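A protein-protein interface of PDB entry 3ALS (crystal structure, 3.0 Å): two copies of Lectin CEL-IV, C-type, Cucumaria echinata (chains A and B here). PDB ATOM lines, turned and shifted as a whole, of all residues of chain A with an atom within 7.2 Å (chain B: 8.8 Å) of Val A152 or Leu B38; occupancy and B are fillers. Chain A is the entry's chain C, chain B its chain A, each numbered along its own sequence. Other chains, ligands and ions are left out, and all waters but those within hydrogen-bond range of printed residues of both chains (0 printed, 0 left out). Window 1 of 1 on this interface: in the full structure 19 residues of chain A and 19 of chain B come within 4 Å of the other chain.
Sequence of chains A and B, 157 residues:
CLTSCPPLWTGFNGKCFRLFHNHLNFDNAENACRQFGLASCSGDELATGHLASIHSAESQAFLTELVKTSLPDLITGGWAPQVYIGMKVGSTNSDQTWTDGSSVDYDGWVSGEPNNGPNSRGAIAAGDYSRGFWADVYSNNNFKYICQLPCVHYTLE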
ATOM      1  N   GLY A  14      29.351 -26.248 -13.309  1.00  0.00           N
ATOM      2  CA  GLY A  14      28.578 -26.102 -14.531  1.00  0.00           C
ATOM      3  C   GLY A  14      27.084 -26.359 -14.453  1.00  0.00           C
ATOM      4  O   GLY A  14      26.386 -26.182 -15.451  1.00  0.00           O
ATOM      5  N   LYS A  15      26.594 -26.808 -13.297  1.00  0.00           N
ATOM      6  CA  LYS A  15      25.152 -26.871 -13.093  1.00  0.00           C
ATOM      7  C   LYS A  15      24.788 -25.830 -12.082  1.00  0.00           C
ATOM      8  O   LYS A  15      25.618 -25.460 -11.238  1.00  0.00           O
ATOM      9  CB  LYS A  15      24.698 -28.222 -12.577  1.00  0.00           C
ATOM     10  CG  LYS A  15      25.044 -29.385 -13.426  1.00  0.00           C
ATOM     11  CD  LYS A  15      24.898 -30.644 -12.588  1.00  0.00           C
ATOM     12  CE  LYS A  15      23.441 -31.089 -12.506  1.00  0.00           C
ATOM     13  NZ  LYS A  15      23.363 -32.468 -11.907  1.00  0.00           N
ATOM     14  N   LEU A  38      15.134 -23.882 -20.551  1.00  0.00           N
ATOM     15  CA  LEU A  38      16.192 -23.330 -21.358  1.00  0.00           C
ATOM     16  C   LEU A  38      15.548 -23.281 -22.711  1.00  0.00           C
ATOM     17  O   LEU A  38      15.005 -24.303 -23.165  1.00  0.00           O
ATOM     18  CB  LEU A  38      17.303 -24.339 -21.378  1.00  0.00           C
ATOM     19  CG  LEU A  38      18.752 -24.138 -21.789  1.00  0.00           C
ATOM     20  CD1 LEU A  38      18.983 -24.723 -23.142  1.00  0.00           C
ATOM     21  CD2 LEU A  38      19.200 -22.687 -21.684  1.00  0.00           C
ATOM     22  N   LEU A  46      13.674 -25.800 -25.197  1.00  0.00           N
ATOM     23  CA  LEU A  46      14.624 -26.891 -25.533  1.00  0.00           C
ATOM     24  C   LEU A  46      14.747 -27.952 -24.472  1.00  0.00           C
ATOM     25  O   LEU A  46      15.057 -29.110 -24.800  1.00  0.00           O
ATOM     26  CB  LEU A  46      16.036 -26.379 -25.811  1.00  0.00           C
ATOM     27  CG  LEU A  46      16.144 -25.496 -27.037  1.00  0.00           C
ATOM     28  CD1 LEU A  46      17.511 -24.915 -27.168  1.00  0.00           C
ATOM     29  CD2 LEU A  46      15.807 -26.351 -28.210  1.00  0.00           C
ATOM     30  N   ALA A  47      14.535 -27.549 -23.207  1.00  0.00           N
ATOM     31  CA  ALA A  47      14.729 -28.407 -22.039  1.00  0.00           C
ATOM     32  C   ALA A  47      14.124 -27.780 -20.796  1.00  0.00           C
ATOM     33  O   ALA A  47      13.789 -26.596 -20.776  1.00  0.00           O
ATOM     34  CB  ALA A  47      16.192 -28.656 -21.822  1.00  0.00           C
ATOM     35  N   LEU A 149      18.867 -26.172 -12.789  1.00  0.00           N
ATOM     36  CA  LEU A 149      18.490 -25.691 -14.109  1.00  0.00           C
ATOM     37  C   LEU A 149      18.975 -26.633 -15.179  1.00  0.00           C
ATOM     38  O   LEU A 149      19.942 -27.327 -14.955  1.00  0.00           O
ATOM     39  CB  LEU A 149      19.125 -24.344 -14.361  1.00  0.00           C
ATOM     40  CG  LEU A 149      18.480 -23.238 -13.565  1.00  0.00           C
ATOM     41  CD1 LEU A 149      19.322 -22.016 -13.761  1.00  0.00           C
ATOM     42  CD2 LEU A 149      17.010 -23.087 -14.010  1.00  0.00           C
ATOM     43  N   PRO A 150      18.341 -26.621 -16.363  1.00  0.00           N
ATOM     44  CA  PRO A 150      18.743 -27.594 -17.397  1.00  0.00           C
ATOM     45  C   PRO A 150      20.269 -27.674 -17.612  1.00  0.00           C
ATOM     46  O   PRO A 150      20.951 -26.653 -17.724  1.00  0.00           O
ATOM     47  CB  PRO A 150      18.041 -27.092 -18.655  1.00  0.00           C
ATOM     48  CG  PRO A 150      16.936 -26.283 -18.162  1.00  0.00           C
ATOM     49  CD  PRO A 150      17.363 -25.652 -16.872  1.00  0.00           C
ATOM     50  N   CYS A 151      20.774 -28.900 -17.616  1.00  0.00           N
ATOM     51  CA  CYS A 151      22.170 -29.146 -17.727  1.00  0.00           C
ATOM     52  C   CYS A 151      22.551 -29.314 -19.218  1.00  0.00           C
ATOM     53  O   CYS A 151      22.007 -30.183 -19.920  1.00  0.00           O
ATOM     54  CB  CYS A 151      22.474 -30.390 -16.910  1.00  0.00           C
ATOM     55  SG  CYS A 151      24.275 -30.576 -16.658  1.00  0.00           S
ATOM     56  N   VAL A 152      23.474 -28.484 -19.698  1.00  0.00           N
ATOM     57  CA  VAL A 152      23.837 -28.454 -21.115  1.00  0.00           C
ATOM     58  C   VAL A 152      25.315 -28.105 -21.302  1.00  0.00           C
ATOM     59  O   VAL A 152      25.931 -27.409 -20.491  1.00  0.00           O
ATOM     60  CB  VAL A 152      22.996 -27.439 -21.901  1.00  0.00           C
ATOM     61  CG1 VAL A 152      21.567 -27.869 -21.973  1.00  0.00           C
ATOM     62  CG2 VAL A 152      23.201 -25.908 -21.401  1.00  0.00           C
ATOM     63  N   HIS A 153      25.897 -28.607 -22.375  1.00  0.00           N
ATOM     64  CA  HIS A 153      27.265 -28.256 -22.723  1.00  0.00           C
ATOM     65  C   HIS A 153      27.387 -28.215 -24.255  1.00  0.00           C
ATOM     66  O   HIS A 153      26.573 -28.848 -24.973  1.00  0.00           O
ATOM     67  CB  HIS A 153      28.255 -29.238 -22.076  1.00  0.00           C
ATOM     68  CG  HIS A 153      28.152 -30.633 -22.610  1.00  0.00           C
ATOM     69  ND1 HIS A 153      27.106 -31.478 -22.297  1.00  0.00           N
ATOM     70  CD2 HIS A 153      28.955 -31.329 -23.453  1.00  0.00           C
ATOM     71  CE1 HIS A 153      27.263 -32.636 -22.919  1.00  0.00           C
ATOM     72  NE2 HIS A 153      28.379 -32.571 -23.625  1.00  0.00           N
ATOM     73  N   TYR A 154      28.377 -27.455 -24.744  1.00  0.00           N
ATOM     74  CA  TYR A 154      28.629 -27.332 -26.163  1.00  0.00           C
ATOM     75  C   TYR A 154      29.295 -28.592 -26.609  1.00  0.00           C
ATOM     76  O   TYR A 154      30.102 -29.104 -25.876  1.00  0.00           O
ATOM     77  CB  TYR A 154      29.557 -26.178 -26.385  1.00  0.00           C
ATOM     78  CG  TYR A 154      28.892 -24.876 -26.183  1.00  0.00           C
ATOM     79  CD1 TYR A 154      27.650 -24.624 -26.744  1.00  0.00           C
ATOM     80  CD2 TYR A 154      29.489 -23.902 -25.431  1.00  0.00           C
ATOM     81  CE1 TYR A 154      27.030 -23.401 -26.562  1.00  0.00           C
ATOM     82  CE2 TYR A 154      28.886 -22.686 -25.226  1.00  0.00           C
ATOM     83  CZ  TYR A 154      27.658 -22.424 -25.801  1.00  0.00           C
ATOM     84  OH  TYR A 154      27.056 -21.200 -25.613  1.00  0.00           O
ATOM     85  N   THR A 155      28.927 -29.111 -27.774  1.00  0.00           N
ATOM     86  CA  THR A 155      29.594 -30.246 -28.394  1.00  0.00           C
ATOM     87  C   THR A 155      30.477 -29.730 -29.519  1.00  0.00           C
ATOM     88  O   THR A 155      29.942 -29.251 -30.505  1.00  0.00           O
ATOM     89  CB  THR A 155      28.563 -31.291 -29.019  1.00  0.00           C
ATOM     90  OG1 THR A 155      27.411 -30.655 -29.608  1.00  0.00           O
ATOM     91  CG2 THR A 155      28.086 -32.261 -28.004  1.00  0.00           C
ATOM     92  N   CYS B  33      29.464 -25.547 -39.557  1.00  0.00           N
ATOM     93  CA  CYS B  33      29.013 -24.953 -38.344  1.00  0.00           C
ATOM     94  C   CYS B  33      28.087 -25.881 -37.584  1.00  0.00           C
ATOM     95  O   CYS B  33      28.110 -25.921 -36.345  1.00  0.00           O
ATOM     96  CB  CYS B  33      28.277 -23.679 -38.635  1.00  0.00           C
ATOM     97  SG  CYS B  33      29.241 -22.304 -39.261  1.00  0.00           S
ATOM     98  N   ARG B  34      27.270 -26.626 -38.302  1.00  0.00           N
ATOM     99  CA  ARG B  34      26.396 -27.578 -37.648  1.00  0.00           C
ATOM    100  C   ARG B  34      27.100 -28.764 -36.968  1.00  0.00           C
ATOM    101  O   ARG B  34      26.439 -29.633 -36.355  1.00  0.00           O
ATOM    102  CB  ARG B  34      25.402 -28.130 -38.643  1.00  0.00           C
ATOM    103  CG  ARG B  34      24.646 -27.077 -39.317  1.00  0.00           C
ATOM    104  CD  ARG B  34      23.468 -27.676 -39.898  1.00  0.00           C
ATOM    105  NE  ARG B  34      22.696 -26.614 -40.512  1.00  0.00           N
ATOM    106  CZ  ARG B  34      21.679 -26.832 -41.341  1.00  0.00           C
ATOM    107  NH1 ARG B  34      21.350 -28.078 -41.661  1.00  0.00           N
ATOM    108  NH2 ARG B  34      21.008 -25.813 -41.858  1.00  0.00           N
ATOM    109  N   GLN B  35      28.427 -28.839 -37.092  1.00  0.00           N
ATOM    110  CA  GLN B  35      29.137 -29.938 -36.477  1.00  0.00           C
ATOM    111  C   GLN B  35      29.247 -29.613 -34.995  1.00  0.00           C
ATOM    112  O   GLN B  35      29.285 -30.534 -34.174  1.00  0.00           O
ATOM    113  CB  GLN B  35      30.475 -30.210 -37.184  1.00  0.00           C
ATOM    114  CG  GLN B  35      30.354 -30.602 -38.656  1.00  0.00           C
ATOM    115  CD  GLN B  35      29.228 -31.648 -38.925  1.00  0.00           C
ATOM    116  OE1 GLN B  35      29.357 -32.835 -38.630  1.00  0.00           O
ATOM    117  NE2 GLN B  35      28.126 -31.191 -39.499  1.00  0.00           N
ATOM    118  N   PHE B  36      29.227 -28.319 -34.662  1.00  0.00           N
ATOM    119  CA  PHE B  36      29.107 -27.876 -33.289  1.00  0.00           C
ATOM    120  C   PHE B  36      27.671 -27.909 -32.786  1.00  0.00           C
ATOM    121  O   PHE B  36      26.746 -27.691 -33.560  1.00  0.00           O
ATOM    122  CB  PHE B  36      29.696 -26.502 -33.148  1.00  0.00           C
ATOM    123  CG  PHE B  36      31.071 -26.377 -33.776  1.00  0.00           C
ATOM    124  CD1 PHE B  36      32.203 -26.927 -33.166  1.00  0.00           C
ATOM    125  CD2 PHE B  36      31.244 -25.711 -34.977  1.00  0.00           C
ATOM    126  CE1 PHE B  36      33.474 -26.827 -33.751  1.00  0.00           C
ATOM    127  CE2 PHE B  36      32.523 -25.607 -35.547  1.00  0.00           C
ATOM    128  CZ  PHE B  36      33.634 -26.173 -34.922  1.00  0.00           C
ATOM    129  N   GLY B  37      27.461 -28.216 -31.505  1.00  0.00           N
ATOM    130  CA  GLY B  37      26.094 -28.327 -30.962  1.00  0.00           C
ATOM    131  C   GLY B  37      25.943 -27.993 -29.493  1.00  0.00           C
ATOM    132  O   GLY B  37      26.865 -27.506 -28.842  1.00  0.00           O
ATOM    133  N   LEU B  38      24.765 -28.252 -28.961  1.00  0.00           N
ATOM    134  CA  LEU B  38      24.510 -28.098 -27.537  1.00  0.00           C
ATOM    135  C   LEU B  38      23.778 -29.371 -27.183  1.00  0.00           C
ATOM    136  O   LEU B  38      22.765 -29.712 -27.837  1.00  0.00           O
ATOM    137  CB  LEU B  38      23.615 -26.907 -27.367  1.00  0.00           C
ATOM    138  CG  LEU B  38      23.440 -26.050 -26.156  1.00  0.00           C
ATOM    139  CD1 LEU B  38      22.124 -26.375 -25.607  1.00  0.00           C
ATOM    140  CD2 LEU B  38      24.550 -26.180 -25.196  1.00  0.00           C
ATOM    141  N   ALA B  39      24.294 -30.120 -26.208  1.00  0.00           N
ATOM    142  CA  ALA B  39      23.555 -31.296 -25.733  1.00  0.00           C
ATOM    143  C   ALA B  39      23.214 -31.187 -24.247  1.00  0.00           C
ATOM    144  O   ALA B  39      23.877 -30.431 -23.488  1.00  0.00           O
ATOM    145  CB  ALA B  39      24.327 -32.543 -25.995  1.00  0.00           C
ATOM    146  N   SER B  40      22.185 -31.928 -23.820  1.00  0.00           N
ATOM    147  CA  SER B  40      21.942 -32.023 -22.367  1.00  0.00           C
ATOM    148  C   SER B  40      23.027 -32.895 -21.777  1.00  0.00           C
ATOM    149  O   SER B  40      23.521 -33.786 -22.449  1.00  0.00           O
ATOM    150  CB  SER B  40      20.519 -32.537 -21.994  1.00  0.00           C
ATOM    151  OG  SER B  40      20.488 -33.949 -22.040  1.00  0.00           O
ATOM    152  N   CYS B  41      23.407 -32.638 -20.538  1.00  0.00           N
ATOM    153  CA  CYS B  41      24.247 -33.593 -19.818  1.00  0.00           C
ATOM    154  C   CYS B  41      23.733 -35.066 -19.839  1.00  0.00           C
ATOM    155  O   CYS B  41      24.557 -35.945 -20.018  1.00  0.00           O
ATOM    156  CB  CYS B  41      24.482 -33.105 -18.401  1.00  0.00           C
ATOM    157  SG  CYS B  41      25.021 -31.398 -18.415  1.00  0.00           S
ATOM    158  N   SER B  42      22.413 -35.323 -19.676  1.00  0.00           N
ATOM    159  CA  SER B  42      21.805 -36.653 -19.944  1.00  0.00           C
ATOM    160  C   SER B  42      22.349 -37.315 -21.244  1.00  0.00           C
ATOM    161  O   SER B  42      22.341 -38.543 -21.357  1.00  0.00           O
ATOM    162  CB  SER B  42      20.256 -36.621 -20.084  1.00  0.00           C
ATOM    163  OG  SER B  42      19.601 -35.695 -19.240  1.00  0.00           O
ATOM    164  N   GLY B  43      22.765 -36.520 -22.236  1.00  0.00           N
ATOM    165  CA  GLY B  43      23.220 -37.069 -23.498  1.00  0.00           C
ATOM    166  C   GLY B  43      22.522 -36.620 -24.787  1.00  0.00           C
ATOM    167  O   GLY B  43      23.141 -36.719 -25.826  1.00  0.00           O
ATOM    168  N   ASP B  44      21.266 -36.130 -24.756  1.00  0.00           N
ATOM    169  CA  ASP B  44      20.477 -35.805 -25.992  1.00  0.00           C
ATOM    170  C   ASP B  44      20.958 -34.533 -26.699  1.00  0.00           C
ATOM    171  O   ASP B  44      21.156 -33.498 -26.038  1.00  0.00           O
ATOM    172  CB  ASP B  44      18.956 -35.643 -25.708  1.00  0.00           C
ATOM    173  CG  ASP B  44      18.455 -36.495 -24.509  1.00  0.00           C
ATOM    174  OD1 ASP B  44      17.847 -37.548 -24.748  1.00  0.00           O
ATOM    175  OD2 ASP B  44      18.663 -36.147 -23.320  1.00  0.00           O
ATOM    176  N   GLU B  45      21.113 -34.604 -28.032  1.00  0.00           N
ATOM    177  CA  GLU B  45      21.425 -33.433 -28.864  1.00  0.00           C
ATOM    178  C   GLU B  45      20.230 -32.467 -28.815  1.00  0.00           C
ATOM    179  O   GLU B  45      19.107 -32.876 -29.034  1.00  0.00           O
ATOM    180  CB  GLU B  45      21.838 -33.845 -30.301  1.00  0.00           C
ATOM    181  CG  GLU B  45      21.686 -32.713 -31.384  1.00  0.00           C
ATOM    182  CD  GLU B  45      22.969 -32.413 -32.232  1.00  0.00           C
ATOM    183  OE1 GLU B  45      23.150 -33.020 -33.315  1.00  0.00           O
ATOM    184  OE2 GLU B  45      23.787 -31.540 -31.841  1.00  0.00           O
ATOM    185  N   LEU B  46      20.477 -31.197 -28.480  1.00  0.00           N
ATOM    186  CA  LEU B  46      19.387 -30.226 -28.311  1.00  0.00           C
ATOM    187  C   LEU B  46      19.286 -29.207 -29.408  1.00  0.00           C
ATOM    188  O   LEU B  46      18.188 -28.719 -29.699  1.00  0.00           O
ATOM    189  CB  LEU B  46      19.491 -29.486 -26.978  1.00  0.00           C
ATOM    190  CG  LEU B  46      19.305 -30.379 -25.763  1.00  0.00           C
ATOM    191  CD1 LEU B  46      19.428 -29.525 -24.576  1.00  0.00           C
ATOM    192  CD2 LEU B  46      17.945 -31.036 -25.772  1.00  0.00           C
ATOM    193  N   ALA B  47      20.436 -28.865 -29.978  1.00  0.00           N
ATOM    194  CA  ALA B  47      20.532 -27.832 -30.991  1.00  0.00           C
ATOM    195  C   ALA B  47      21.890 -27.840 -31.681  1.00  0.00           C
ATOM    196  O   ALA B  47      22.820 -28.542 -31.283  1.00  0.00           O
ATOM    197  CB  ALA B  47      20.282 -26.486 -30.389  1.00  0.00           C
ATOM    198  N   THR B  48      21.998 -27.008 -32.710  1.00  0.00           N
ATOM    199  CA  THR B  48      23.121 -27.034 -33.647  1.00  0.00           C
ATOM    200  C   THR B  48      23.684 -25.652 -33.771  1.00  0.00           C
ATOM    201  O   THR B  48      22.954 -24.697 -33.578  1.00  0.00           O
ATOM    202  CB  THR B  48      22.546 -27.467 -34.960  1.00  0.00           C
ATOM    203  OG1 THR B  48      22.729 -28.858 -35.029  1.00  0.00           O
ATOM    204  CG2 THR B  48      23.167 -26.813 -36.139  1.00  0.00           C
ATOM    205  N   GLY B  49      24.976 -25.540 -34.056  1.00  0.00           N
ATOM    206  CA  GLY B  49      25.587 -24.254 -34.498  1.00  0.00           C
ATOM    207  C   GLY B  49      25.130 -23.828 -35.906  1.00  0.00           C
ATOM    208  O   GLY B  49      24.505 -24.600 -36.657  1.00  0.00           O
ATOM    209  N   LEU B 149      27.875 -20.560 -32.002  1.00  0.00           N
ATOM    210  CA  LEU B 149      27.372 -21.729 -31.269  1.00  0.00           C
ATOM    211  C   LEU B 149      25.920 -21.532 -30.968  1.00  0.00           C
ATOM    212  O   LEU B 149      25.467 -20.404 -30.916  1.00  0.00           O
ATOM    213  CB  LEU B 149      28.130 -21.897 -29.968  1.00  0.00           C
ATOM    214  CG  LEU B 149      29.558 -22.347 -30.191  1.00  0.00           C
ATOM    215  CD1 LEU B 149      30.317 -22.264 -28.881  1.00  0.00           C
ATOM    216  CD2 LEU B 149      29.504 -23.764 -30.748  1.00  0.00           C
ATOM    217  N   PRO B 150      25.185 -22.610 -30.712  1.00  0.00           N
ATOM    218  CA  PRO B 150      23.735 -22.460 -30.456  1.00  0.00           C
ATOM    219  C   PRO B 150      23.391 -21.358 -29.431  1.00  0.00           C
ATOM    220  O   PRO B 150      24.018 -21.222 -28.367  1.00  0.00           O
ATOM    221  CB  PRO B 150      23.303 -23.830 -29.961  1.00  0.00           C
ATOM    222  CG  PRO B 150      24.355 -24.759 -30.437  1.00  0.00           C
ATOM    223  CD  PRO B 150      25.649 -23.978 -30.464  1.00  0.00           C
ATOM    224  N   CYS B 151      22.411 -20.548 -29.801  1.00  0.00           N
ATOM    225  CA  CYS B 151      21.994 -19.446 -28.994  1.00  0.00           C
ATOM    226  C   CYS B 151      20.867 -19.877 -28.068  1.00  0.00           C
ATOM    227  O   CYS B 151      19.798 -20.355 -28.502  1.00  0.00           O
ATOM    228  CB  CYS B 151      21.463 -18.357 -29.892  1.00  0.00           C
ATOM    229  SG  CYS B 151      21.279 -16.793 -28.978  1.00  0.00           S
ATOM    230  N   VAL B 152      21.070 -19.637 -26.781  1.00  0.00           N
ATOM    231  CA  VAL B 152      20.220 -20.251 -25.790  1.00  0.00           C
ATOM    232  C   VAL B 152      20.194 -19.373 -24.526  1.00  0.00           C
ATOM    233  O   VAL B 152      21.227 -18.762 -24.157  1.00  0.00           O
ATOM    234  CB  VAL B 152      20.863 -21.585 -25.598  1.00  0.00           C
ATOM    235  CG1 VAL B 152      21.725 -21.694 -24.380  1.00  0.00           C
ATOM    236  CG2 VAL B 152      20.067 -22.737 -26.098  1.00  0.00           C
ATOM    237  N   HIS B 153      19.015 -19.259 -23.899  1.00  0.00           N
ATOM    238  CA  HIS B 153      18.864 -18.510 -22.624  1.00  0.00           C
ATOM    239  C   HIS B 153      17.910 -19.269 -21.697  1.00  0.00           C
ATOM    240  O   HIS B 153      17.097 -20.100 -22.150  1.00  0.00           O
ATOM    241  CB  HIS B 153      18.412 -17.054 -22.834  1.00  0.00           C
ATOM    242  CG  HIS B 153      17.035 -16.927 -23.401  1.00  0.00           C
ATOM    243  ND1 HIS B 153      16.748 -17.183 -24.726  1.00  0.00           N
ATOM    244  CD2 HIS B 153      15.857 -16.595 -22.827  1.00  0.00           C
ATOM    245  CE1 HIS B 153      15.452 -17.026 -24.952  1.00  0.00           C
ATOM    246  NE2 HIS B 153      14.888 -16.670 -23.812  1.00  0.00           N
ATOM    247  N   TYR B 154      18.041 -19.015 -20.396  1.00  0.00           N
ATOM    248  CA  TYR B 154      17.111 -19.573 -19.405  1.00  0.00           C
ATOM    249  C   TYR B 154      15.799 -18.864 -19.453  1.00  0.00           C
ATOM    250  O   TYR B 154      15.810 -17.655 -19.656  1.00  0.00           O
ATOM    251  CB  TYR B 154      17.642 -19.380 -18.020  1.00  0.00           C
ATOM    252  CG  TYR B 154      18.808 -20.239 -17.762  1.00  0.00           C
ATOM    253  CD1 TYR B 154      18.753 -21.589 -18.007  1.00  0.00           C
ATOM    254  CD2 TYR B 154      19.972 -19.714 -17.286  1.00  0.00           C
ATOM    255  CE1 TYR B 154      19.866 -22.411 -17.782  1.00  0.00           C
ATOM    256  CE2 TYR B 154      21.089 -20.515 -17.048  1.00  0.00           C
ATOM    257  CZ  TYR B 154      21.031 -21.855 -17.306  1.00  0.00           C
ATOM    258  OH  TYR B 154      22.134 -22.618 -17.060  1.00  0.00           O
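Hydrophobic or aromatic side chains of chain A within 4 Å of the printed part of chain B: Leu A38, Leu A46, Leu A149, Val A152, His A153 and Tyr A154.
CD1 of Leu A38 touches CG2 of Val B152, 3.7 Å away. His B153 touches Leu A38 (O to CD2, 3.4 Å). Leu A46 touches Val B152. Ser B40 touches Cys A151 (CA to O, 3.1 Å). CB of Val A152 touches CD2 of Leu B38, 3.9 Å away. Leu B38 touches His A153 (CD2 to O, 3.4 Å). Gly B37 touches Tyr A154. CD2 of Leu B38 touches CD1 of Tyr A154, at 3.8 Å. Gln B35 touches Thr A155. Thr A155 touches Leu B38 (OG1 to N, 3.6 Å).
Of the printed residues of chain B, Leu A38 touches Val B152 (3.7 Å), His B153 (3.4 Å) and Tyr B154 (3.9 Å). Of chain A, only Val A152 (3.9 Å), His A153 (3.4 Å), Tyr A154 (3.8 Å) and Thr A155 (3.6 Å) come within 4 Å of Leu B38. Of the printed residues of chain A, Tyr B154 touches Leu A38 (3.9 Å) and Leu A149 (3.9 Å). The nearest residue of chain B that does not touch Val A152 is Ser B40 (4.2 Å). The nearest residue of chain A that does not touch Leu B38 is Leu A38 (4.3 Å).
Leu A38 touches Val B152, and with the chains exchanged Val A152 touches Leu B38. Leu A38 touches Tyr B154, and with the chains exchanged Tyr A154 touches Leu B38. Leu A46 touches Val B152, and with the chains exchanged Val A152 touches Leu B46. Leu A149 touches Tyr B154, and with the chains exchanged Tyr A154 touches Leu B149. Of the 22 pairs that touch across the chains among the printed residues, 11 have their exchanged pair printed and touching as well.
The backbone carbonyl oxygen (O) of Phe B36 lies within hydrogen-bond range of the backbone NH (N) of Gly B49 (2.8 Å). The backbone carbonyl oxygen (O) of Ala B47 is in hydrogen-bond range of the backbone NH (N) of Leu B38 (3.0 Å). OG of Ser B40 lies close to N of Ser B42. O of Ala A47 sits at hydrogen-bond distance from N of Leu A38 (3.0 Å). The side-chain hydroxyl (OG) of Ser B40 is in hydrogen-bond range of the backbone NH (N) of Gly B43 (3.4 Å). O of Leu A38 lies within hydrogen-bond range of N of Leu A46 (2.9 Å).
The side-chain sulfur of Cys B41 lies within hydrogen-bond range of the backbone NH of Val A152, at 3.5 Å. O of Gly B37 is in hydrogen-bond range of N of Thr A155 (2.8 Å). The side-chain sulfur (SG) of Cys A151 forms a disulfide with the side-chain sulfur (SG) of Cys B41, 2.1 Å away. The backbone NH (N) of Ala B39 lies within hydrogen-bond range of the backbone carbonyl oxygen (O) of His A153, 2.9 Å away.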
